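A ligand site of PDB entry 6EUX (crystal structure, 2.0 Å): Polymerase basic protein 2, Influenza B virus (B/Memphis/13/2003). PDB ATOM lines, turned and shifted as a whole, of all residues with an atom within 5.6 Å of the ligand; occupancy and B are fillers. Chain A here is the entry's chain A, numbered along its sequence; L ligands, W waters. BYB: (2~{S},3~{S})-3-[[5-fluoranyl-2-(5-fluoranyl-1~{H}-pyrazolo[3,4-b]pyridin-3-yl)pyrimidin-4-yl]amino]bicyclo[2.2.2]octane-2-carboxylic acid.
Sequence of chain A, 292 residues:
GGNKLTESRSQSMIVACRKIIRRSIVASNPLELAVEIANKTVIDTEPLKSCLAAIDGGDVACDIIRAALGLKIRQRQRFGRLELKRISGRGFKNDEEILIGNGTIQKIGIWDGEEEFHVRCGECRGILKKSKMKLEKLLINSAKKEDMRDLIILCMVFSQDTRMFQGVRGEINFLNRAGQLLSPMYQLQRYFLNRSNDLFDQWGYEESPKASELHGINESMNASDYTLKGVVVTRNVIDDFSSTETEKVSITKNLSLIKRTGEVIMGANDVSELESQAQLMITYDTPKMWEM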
ATOM      1  N   GLN A  77     -18.477  17.757   8.186  1.00  0.00           N
ATOM      2  CA  GLN A  77     -19.599  18.706   8.215  1.00  0.00           C
ATOM      3  C   GLN A  77     -19.302  19.815   9.224  1.00  0.00           C
ATOM      4  O   GLN A  77     -18.720  19.561  10.281  1.00  0.00           O
ATOM      5  CB  GLN A  77     -20.892  17.965   8.600  1.00  0.00           C
ATOM      6  CG  GLN A  77     -22.172  18.791   8.508  1.00  0.00           C
ATOM      7  CD  GLN A  77     -22.551  19.167   7.086  1.00  0.00           C
ATOM      8  OE1 GLN A  77     -22.692  18.297   6.227  1.00  0.00           O
ATOM      9  NE2 GLN A  77     -22.724  20.455   6.835  1.00  0.00           N
ATOM     10  N   ARG A  78     -19.686  21.041   8.884  1.00  0.00           N
ATOM     11  CA  ARG A  78     -19.454  22.213   9.716  1.00  0.00           C
ATOM     12  C   ARG A  78     -20.752  22.982   9.968  1.00  0.00           C
ATOM     13  O   ARG A  78     -21.608  23.067   9.094  1.00  0.00           O
ATOM     14  CB  ARG A  78     -18.443  23.159   9.063  1.00  0.00           C
ATOM     15  CG  ARG A  78     -17.042  22.583   8.879  1.00  0.00           C
ATOM     16  CD  ARG A  78     -16.361  22.255  10.200  1.00  0.00           C
ATOM     17  NE  ARG A  78     -16.355  23.405  11.107  1.00  0.00           N
ATOM     18  CZ  ARG A  78     -15.272  23.976  11.660  1.00  0.00           C
ATOM     19  NH1 ARG A  78     -14.033  23.524  11.448  1.00  0.00           N
ATOM     20  NH2 ARG A  78     -15.442  25.028  12.454  1.00  0.00           N
ATOM     21  N   PHE A  79     -20.876  23.520  11.181  1.00  0.00           N
ATOM     22  CA  PHE A  79     -21.966  24.402  11.555  1.00  0.00           C
ATOM     23  C   PHE A  79     -21.386  25.437  12.528  1.00  0.00           C
ATOM     24  O   PHE A  79     -21.382  25.228  13.746  1.00  0.00           O
ATOM     25  CB  PHE A  79     -23.104  23.584  12.170  1.00  0.00           C
ATOM     26  CG  PHE A  79     -24.281  24.417  12.599  1.00  0.00           C
ATOM     27  CD1 PHE A  79     -24.919  25.268  11.689  1.00  0.00           C
ATOM     28  CD2 PHE A  79     -24.780  24.330  13.889  1.00  0.00           C
ATOM     29  CE1 PHE A  79     -26.011  26.031  12.079  1.00  0.00           C
ATOM     30  CE2 PHE A  79     -25.871  25.092  14.280  1.00  0.00           C
ATOM     31  CZ  PHE A  79     -26.494  25.944  13.376  1.00  0.00           C
ATOM     32  N   ARG A  86     -20.472  11.761  10.974  1.00  0.00           N
ATOM     33  CA  ARG A  86     -21.465  10.685  11.143  1.00  0.00           C
ATOM     34  C   ARG A  86     -20.957   9.486  11.932  1.00  0.00           C
ATOM     35  O   ARG A  86     -19.895   8.961  11.623  1.00  0.00           O
ATOM     36  CB  ARG A  86     -21.891  10.204   9.744  1.00  0.00           C
ATOM     37  CG  ARG A  86     -22.876   9.044   9.707  1.00  0.00           C
ATOM     38  CD  ARG A  86     -24.235   9.445  10.205  1.00  0.00           C
ATOM     39  NE  ARG A  86     -24.850  10.487   9.374  1.00  0.00           N
ATOM     40  CZ  ARG A  86     -26.084  10.957   9.538  1.00  0.00           C
ATOM     41  NH1 ARG A  86     -26.852  10.480  10.510  1.00  0.00           N
ATOM     42  NH2 ARG A  86     -26.547  11.905   8.741  1.00  0.00           N
ATOM     43  N   GLY A  91     -30.235  11.128   8.130  1.00  0.00           N
ATOM     44  CA  GLY A  91     -31.083  12.298   8.293  1.00  0.00           C
ATOM     45  C   GLY A  91     -31.708  12.686   6.964  1.00  0.00           C
ATOM     46  O   GLY A  91     -31.092  12.518   5.911  1.00  0.00           O
ATOM     47  N   LYS A  93     -34.162  16.039   5.339  1.00  0.00           N
ATOM     48  CA  LYS A  93     -34.609  17.394   5.599  1.00  0.00           C
ATOM     49  C   LYS A  93     -35.960  17.646   4.934  1.00  0.00           C
ATOM     50  O   LYS A  93     -36.116  17.396   3.741  1.00  0.00           O
ATOM     51  CB  LYS A  93     -33.587  18.402   5.057  1.00  0.00           C
ATOM     52  CG  LYS A  93     -33.813  19.841   5.505  1.00  0.00           C
ATOM     53  CD  LYS A  93     -32.681  20.760   5.070  1.00  0.00           C
ATOM     54  CE  LYS A  93     -32.777  21.103   3.593  1.00  0.00           C
ATOM     55  NZ  LYS A  93     -31.719  22.089   3.215  1.00  0.00           N
ATOM     56  N   GLY A 109     -35.680  24.073   7.475  1.00  0.00           N
ATOM     57  CA  GLY A 109     -35.372  22.703   7.064  1.00  0.00           C
ATOM     58  C   GLY A 109     -35.162  21.841   8.299  1.00  0.00           C
ATOM     59  O   GLY A 109     -34.077  21.861   8.889  1.00  0.00           O
ATOM     60  N   TRP A 111     -34.715  18.334  10.153  1.00  0.00           N
ATOM     61  CA  TRP A 111     -34.145  17.020   9.873  1.00  0.00           C
ATOM     62  C   TRP A 111     -34.849  15.927  10.679  1.00  0.00           C
ATOM     63  O   TRP A 111     -35.117  16.103  11.872  1.00  0.00           O
ATOM     64  CB  TRP A 111     -32.636  17.022  10.135  1.00  0.00           C
ATOM     65  CG  TRP A 111     -31.897  17.868   9.153  1.00  0.00           C
ATOM     66  CD1 TRP A 111     -31.727  19.225   9.209  1.00  0.00           C
ATOM     67  CD2 TRP A 111     -31.249  17.438   7.948  1.00  0.00           C
ATOM     68  NE1 TRP A 111     -30.996  19.657   8.131  1.00  0.00           N
ATOM     69  CE2 TRP A 111     -30.689  18.591   7.336  1.00  0.00           C
ATOM     70  CE3 TRP A 111     -31.065  16.187   7.332  1.00  0.00           C
ATOM     71  CZ2 TRP A 111     -29.975  18.521   6.130  1.00  0.00           C
ATOM     72  CZ3 TRP A 111     -30.341  16.125   6.132  1.00  0.00           C
ATOM     73  CH2 TRP A 111     -29.818  17.286   5.548  1.00  0.00           C
ATOM     74  N   GLU A 115     -30.149   9.819  14.823  1.00  0.00           N
ATOM     75  CA  GLU A 115     -28.782  10.030  14.335  1.00  0.00           C
ATOM     76  C   GLU A 115     -27.801  10.158  15.489  1.00  0.00           C
ATOM     77  O   GLU A 115     -28.174  10.587  16.590  1.00  0.00           O
ATOM     78  CB  GLU A 115     -28.687  11.299  13.470  1.00  0.00           C
ATOM     79  CG  GLU A 115     -29.715  11.368  12.338  1.00  0.00           C
ATOM     80  CD  GLU A 115     -29.546  12.608  11.459  1.00  0.00           C
ATOM     81  OE1 GLU A 115     -30.326  13.572  11.628  1.00  0.00           O
ATOM     82  OE2 GLU A 115     -28.633  12.602  10.599  1.00  0.00           O
ATOM     83  N   PHE A 117     -23.653  11.658  16.021  1.00  0.00           N
ATOM     84  CA  PHE A 117     -22.504  12.341  15.454  1.00  0.00           C
ATOM     85  C   PHE A 117     -21.360  12.398  16.464  1.00  0.00           C
ATOM     86  O   PHE A 117     -21.576  12.553  17.670  1.00  0.00           O
ATOM     87  CB  PHE A 117     -22.882  13.783  15.075  1.00  0.00           C
ATOM     88  CG  PHE A 117     -23.922  13.881  14.003  1.00  0.00           C
ATOM     89  CD1 PHE A 117     -23.550  13.927  12.659  1.00  0.00           C
ATOM     90  CD2 PHE A 117     -25.270  13.950  14.328  1.00  0.00           C
ATOM     91  CE1 PHE A 117     -24.514  14.024  11.663  1.00  0.00           C
ATOM     92  CE2 PHE A 117     -26.234  14.048  13.332  1.00  0.00           C
ATOM     93  CZ  PHE A 117     -25.852  14.088  11.998  1.00  0.00           C
ATOM     94  N   LYS A 130     -29.283  12.424  18.586  1.00  0.00           N
ATOM     95  CA  LYS A 130     -30.475  13.234  18.379  1.00  0.00           C
ATOM     96  C   LYS A 130     -31.472  12.592  17.418  1.00  0.00           C
ATOM     97  O   LYS A 130     -31.125  11.678  16.663  1.00  0.00           O
ATOM     98  CB  LYS A 130     -30.077  14.643  17.900  1.00  0.00           C
ATOM     99  CG  LYS A 130     -29.289  14.715  16.601  1.00  0.00           C
ATOM    100  CD  LYS A 130     -30.146  14.826  15.341  1.00  0.00           C
ATOM    101  CE  LYS A 130     -30.861  16.163  15.252  1.00  0.00           C
ATOM    102  NZ  LYS A 130     -31.815  16.189  14.111  1.00  0.00           N
ATOM    103  N   VAL A 157     -28.634  23.899  19.322  1.00  0.00           N
ATOM    104  CA  VAL A 157     -29.134  24.540  18.105  1.00  0.00           C
ATOM    105  C   VAL A 157     -29.190  23.533  16.958  1.00  0.00           C
ATOM    106  O   VAL A 157     -30.213  23.407  16.302  1.00  0.00           O
ATOM    107  CB  VAL A 157     -28.292  25.789  17.715  1.00  0.00           C
ATOM    108  CG1 VAL A 157     -28.734  26.362  16.372  1.00  0.00           C
ATOM    109  CG2 VAL A 157     -28.419  26.864  18.800  1.00  0.00           C
ATOM    110  N   PHE A 158     -28.094  22.787  16.764  1.00  0.00           N
ATOM    111  CA  PHE A 158     -28.041  21.741  15.724  1.00  0.00           C
ATOM    112  C   PHE A 158     -29.151  20.696  15.875  1.00  0.00           C
ATOM    113  O   PHE A 158     -29.706  20.262  14.868  1.00  0.00           O
ATOM    114  CB  PHE A 158     -26.672  21.044  15.702  1.00  0.00           C
ATOM    115  CG  PHE A 158     -26.529  20.023  14.601  1.00  0.00           C
ATOM    116  CD1 PHE A 158     -26.079  20.398  13.344  1.00  0.00           C
ATOM    117  CD2 PHE A 158     -26.849  18.694  14.820  1.00  0.00           C
ATOM    118  CE1 PHE A 158     -25.959  19.462  12.325  1.00  0.00           C
ATOM    119  CE2 PHE A 158     -26.722  17.751  13.801  1.00  0.00           C
ATOM    120  CZ  PHE A 158     -26.277  18.136  12.554  1.00  0.00           C
ATOM    121  N   SER A 159     -29.484  20.317  17.102  1.00  0.00           N
ATOM    122  CA  SER A 159     -30.549  19.337  17.354  1.00  0.00           C
ATOM    123  C   SER A 159     -31.953  19.794  16.931  1.00  0.00           C
ATOM    124  O   SER A 159     -32.853  18.956  16.770  1.00  0.00           O
ATOM    125  CB  SER A 159     -30.586  18.921  18.829  1.00  0.00           C
ATOM    126  OG  SER A 159     -31.102  19.965  19.641  1.00  0.00           O
ATOM    127  N   GLN A 160     -32.134  21.101  16.763  1.00  0.00           N
ATOM    128  CA  GLN A 160     -33.409  21.734  16.406  1.00  0.00           C
ATOM    129  C   GLN A 160     -34.472  21.440  17.445  1.00  0.00           C
ATOM    130  O   GLN A 160     -35.670  21.362  17.140  1.00  0.00           O
ATOM    131  CB  GLN A 160     -33.881  21.319  15.003  1.00  0.00           C
ATOM    132  CG  GLN A 160     -32.885  21.661  13.907  1.00  0.00           C
ATOM    133  CD  GLN A 160     -33.338  21.197  12.543  1.00  0.00           C
ATOM    134  OE1 GLN A 160     -33.732  20.042  12.373  1.00  0.00           O
ATOM    135  NE2 GLN A 160     -33.258  22.084  11.565  1.00  0.00           N
ATOM    136  N   MET A 185     -31.262  28.841  10.785  1.00  0.00           N
ATOM    137  CA  MET A 185     -30.348  28.057  11.629  1.00  0.00           C
ATOM    138  C   MET A 185     -29.100  28.836  12.051  1.00  0.00           C
ATOM    139  O   MET A 185     -28.634  28.680  13.190  1.00  0.00           O
ATOM    140  CB  MET A 185     -29.947  26.741  10.939  1.00  0.00           C
ATOM    141  CG  MET A 185     -31.064  25.705  10.878  1.00  0.00           C
ATOM    142  SD  MET A 185     -31.689  25.205  12.494  1.00  0.00           S
ATOM    143  CE  MET A 185     -30.253  24.394  13.177  1.00  0.00           C
ATOM    144  N   TYR A 186     -28.547  29.654  11.156  1.00  0.00           N
ATOM    145  CA  TYR A 186     -27.421  30.526  11.515  1.00  0.00           C
ATOM    146  C   TYR A 186     -27.831  31.728  12.370  1.00  0.00           C
ATOM    147  O   TYR A 186     -27.022  32.222  13.159  1.00  0.00           O
ATOM    148  CB  TYR A 186     -26.636  30.965  10.262  1.00  0.00           C
ATOM    149  CG  TYR A 186     -25.725  29.877   9.747  1.00  0.00           C
ATOM    150  CD1 TYR A 186     -24.460  29.682  10.296  1.00  0.00           C
ATOM    151  CD2 TYR A 186     -26.135  29.027   8.732  1.00  0.00           C
ATOM    152  CE1 TYR A 186     -23.623  28.675   9.836  1.00  0.00           C
ATOM    153  CE2 TYR A 186     -25.307  28.012   8.266  1.00  0.00           C
ATOM    154  CZ  TYR A 186     -24.060  27.842   8.824  1.00  0.00           C
ATOM    155  OH  TYR A 186     -23.247  26.840   8.348  1.00  0.00           O
ATOM    156  N   LYS A 259     -20.496  18.087  -1.570  1.00  0.00           N
ATOM    157  CA  LYS A 259     -20.211  16.659  -1.772  1.00  0.00           C
ATOM    158  C   LYS A 259     -20.745  16.178  -3.133  1.00  0.00           C
ATOM    159  O   LYS A 259     -21.405  16.944  -3.849  1.00  0.00           O
ATOM    160  CB  LYS A 259     -20.827  15.826  -0.645  1.00  0.00           C
ATOM    161  CG  LYS A 259     -20.228  16.126   0.728  1.00  0.00           C
ATOM    162  CD  LYS A 259     -20.758  15.182   1.805  1.00  0.00           C
ATOM    163  CE  LYS A 259     -22.200  15.499   2.174  1.00  0.00           C
ATOM    164  NZ  LYS A 259     -22.674  14.695   3.331  1.00  0.00           N
ATOM    165  N   GLU A 263     -25.276  17.584  -0.805  1.00  0.00           N
ATOM    166  CA  GLU A 263     -25.273  18.189   0.540  1.00  0.00           C
ATOM    167  C   GLU A 263     -23.978  18.970   0.822  1.00  0.00           C
ATOM    168  O   GLU A 263     -22.890  18.414   0.725  1.00  0.00           O
ATOM    169  CB  GLU A 263     -25.461  17.104   1.611  1.00  0.00           C
ATOM    170  CG  GLU A 263     -26.833  16.455   1.626  1.00  0.00           C
ATOM    171  CD  GLU A 263     -26.978  15.393   2.712  1.00  0.00           C
ATOM    172  OE1 GLU A 263     -25.961  14.908   3.242  1.00  0.00           O
ATOM    173  OE2 GLU A 263     -28.136  15.032   3.041  1.00  0.00           O
ATOM    174  N   VAL A 264     -24.118  20.246   1.178  1.00  0.00           N
ATOM    175  CA  VAL A 264     -22.961  21.105   1.490  1.00  0.00           C
ATOM    176  C   VAL A 264     -22.385  20.819   2.872  1.00  0.00           C
ATOM    177  O   VAL A 264     -23.139  20.632   3.839  1.00  0.00           O
ATOM    178  CB  VAL A 264     -23.276  22.627   1.341  1.00  0.00           C
ATOM    179  CG1 VAL A 264     -23.796  22.935  -0.061  1.00  0.00           C
ATOM    180  CG2 VAL A 264     -24.257  23.128   2.405  1.00  0.00           C
ATOM    181  N   ILE A 265     -21.051  20.790   2.964  1.00  0.00           N
ATOM    182  CA  ILE A 265     -20.348  20.456   4.229  1.00  0.00           C
ATOM    183  C   ILE A 265     -19.858  21.677   5.015  1.00  0.00           C
ATOM    184  O   ILE A 265     -19.821  21.628   6.242  1.00  0.00           O
ATOM    185  CB  ILE A 265     -19.173  19.448   4.019  1.00  0.00           C
ATOM    186  CG1 ILE A 265     -18.165  19.945   2.970  1.00  0.00           C
ATOM    187  CG2 ILE A 265     -19.720  18.084   3.639  1.00  0.00           C
ATOM    188  CD1 ILE A 265     -16.787  19.322   3.109  1.00  0.00           C
HETATM  189  C1  BYB L   1     -29.383  19.690  11.434  1.00  0.00           C
HETATM  190  C2  BYB L   1     -29.987  18.762  12.283  1.00  0.00           C
HETATM  191  C4  BYB L   1     -28.685  19.223  10.330  1.00  0.00           C
HETATM  192  C5  BYB L   1     -28.619  17.831  10.114  1.00  0.00           C
HETATM  193  C6  BYB L   1     -29.241  16.954  11.020  1.00  0.00           C
HETATM  194  N3  BYB L   1     -29.902  17.452  12.075  1.00  0.00           N
HETATM  195  N7  BYB L   1     -29.007  15.680  10.565  1.00  0.00           N
HETATM  196  N8  BYB L   1     -28.259  15.731   9.386  1.00  0.00           N
HETATM  197  C9  BYB L   1     -27.983  16.995   9.098  1.00  0.00           C
HETATM  198  C10 BYB L   1     -27.252  17.479   7.902  1.00  0.00           C
HETATM  199  N11 BYB L   1     -27.109  18.801   7.709  1.00  0.00           N
HETATM  200  C12 BYB L   1     -26.487  19.284   6.637  1.00  0.00           C
HETATM  201  C13 BYB L   1     -25.991  18.368   5.686  1.00  0.00           C
HETATM  202  C14 BYB L   1     -26.166  17.005   5.917  1.00  0.00           C
HETATM  203  N15 BYB L   1     -26.804  16.601   7.007  1.00  0.00           N
HETATM  204  N16 BYB L   1     -26.330  20.657   6.419  1.00  0.00           N
HETATM  205  C17 BYB L   1     -26.942  21.658   7.308  1.00  0.00           C
HETATM  206  C18 BYB L   1     -25.953  22.096   8.422  1.00  0.00           C
HETATM  207  C19 BYB L   1     -24.786  22.940   7.826  1.00  0.00           C
HETATM  208  C20 BYB L   1     -25.357  24.164   7.070  1.00  0.00           C
HETATM  209  C21 BYB L   1     -26.888  24.169   7.203  1.00  0.00           C
HETATM  210  C22 BYB L   1     -27.445  22.902   6.519  1.00  0.00           C
HETATM  211  F23 BYB L   1     -29.475  21.020  11.660  1.00  0.00           F
HETATM  212  F24 BYB L   1     -25.350  18.827   4.582  1.00  0.00           F
HETATM  213  C25 BYB L   1     -28.966  22.968   6.393  1.00  0.00           C
HETATM  214  O26 BYB L   1     -29.527  23.924   5.641  1.00  0.00           O
HETATM  215  O27 BYB L   1     -29.702  22.191   6.958  1.00  0.00           O
HETATM  216  C28 BYB L   1     -26.739  22.962   9.440  1.00  0.00           C
HETATM  217  C29 BYB L   1     -27.284  24.221   8.711  1.00  0.00           C
HETATM  218  O   HOH W   1     -31.649  23.114   8.476  1.00  0.00           O
HETATM  219  O   HOH W   2     -27.515  13.833   6.400  1.00  0.00           O
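OE1 of Glu 115 lies within hydrogen-bond range of N7 of the ligand (2.7 Å). A nitrogen (N3) of the ligand lies within hydrogen-bond range of the side-chain amino group of Lys 130. The indole nitrogen (NE1) of Trp 111 is in hydrogen-bond range of an oxygen (O27) of the ligand, 3.1 Å away. O26 of the ligand is in salt-bridge range of NZ of Lys 93, at 3.7 Å.
The side-chain amino group (NZ) of Lys 130 lies within salt-bridge range of the side-chain carboxylate (OE1) of Glu 115. The side-chain carboxylate of Glu 115 lies within salt-bridge range of the guanidinium group of Arg 86, 2.8 Å away. The side-chain carboxylate (OE2) of Glu 115 lies within hydrogen-bond range of the backbone NH (N) of Gly 91. NE2 of Gln 77 is in hydrogen-bond range of O of Val 264 (3.0 Å). N of Trp 111 lies within hydrogen-bond range of OE1 of Gln 160 (3.0 Å). NZ of Lys 259 lies within salt-bridge range of OE1 of Glu 263 (3.3 Å). The side-chain sulfur (SD) of Met 185 is in hydrogen-bond range of the side-chain amide nitrogen (NE2) of Gln 160 (3.6 Å). The side-chain amide nitrogen (NE2) of Gln 160 is in hydrogen-bond range of the backbone carbonyl oxygen (O) of Gly 109, at 2.8 Å.
OE1 of Gln 77 sits close to F24 of the ligand. O of Phe 158 sits close to F23 of the ligand, 3.3 Å away. F24 of the ligand lies close to O of Val 264 (2.9 Å). Merely in contact with the ligand: Arg 78, Phe 79, Phe 117, Gln 160, Met 185, Tyr 186 and Glu 263. Hydrophobic or aromatic side chains that line the ligand: Phe 79, Trp 111, Phe 117, Phe 158 and Met 185. Of the 21 residues printed, 14 come within 4 Å of the ligand. The nearest printed residue that does not touch the ligand is Arg 86 (4.2 Å).
Water W1 bridges an oxygen (O27) of the ligand (2.6 Å) and the backbone carbonyl oxygen (O) of Gly 109 (2.8 Å). Water W2 bridges a nitrogen (N15) of the ligand (2.9 Å) and the guanidinium group (NH2) of Arg 86 (3.2 Å).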
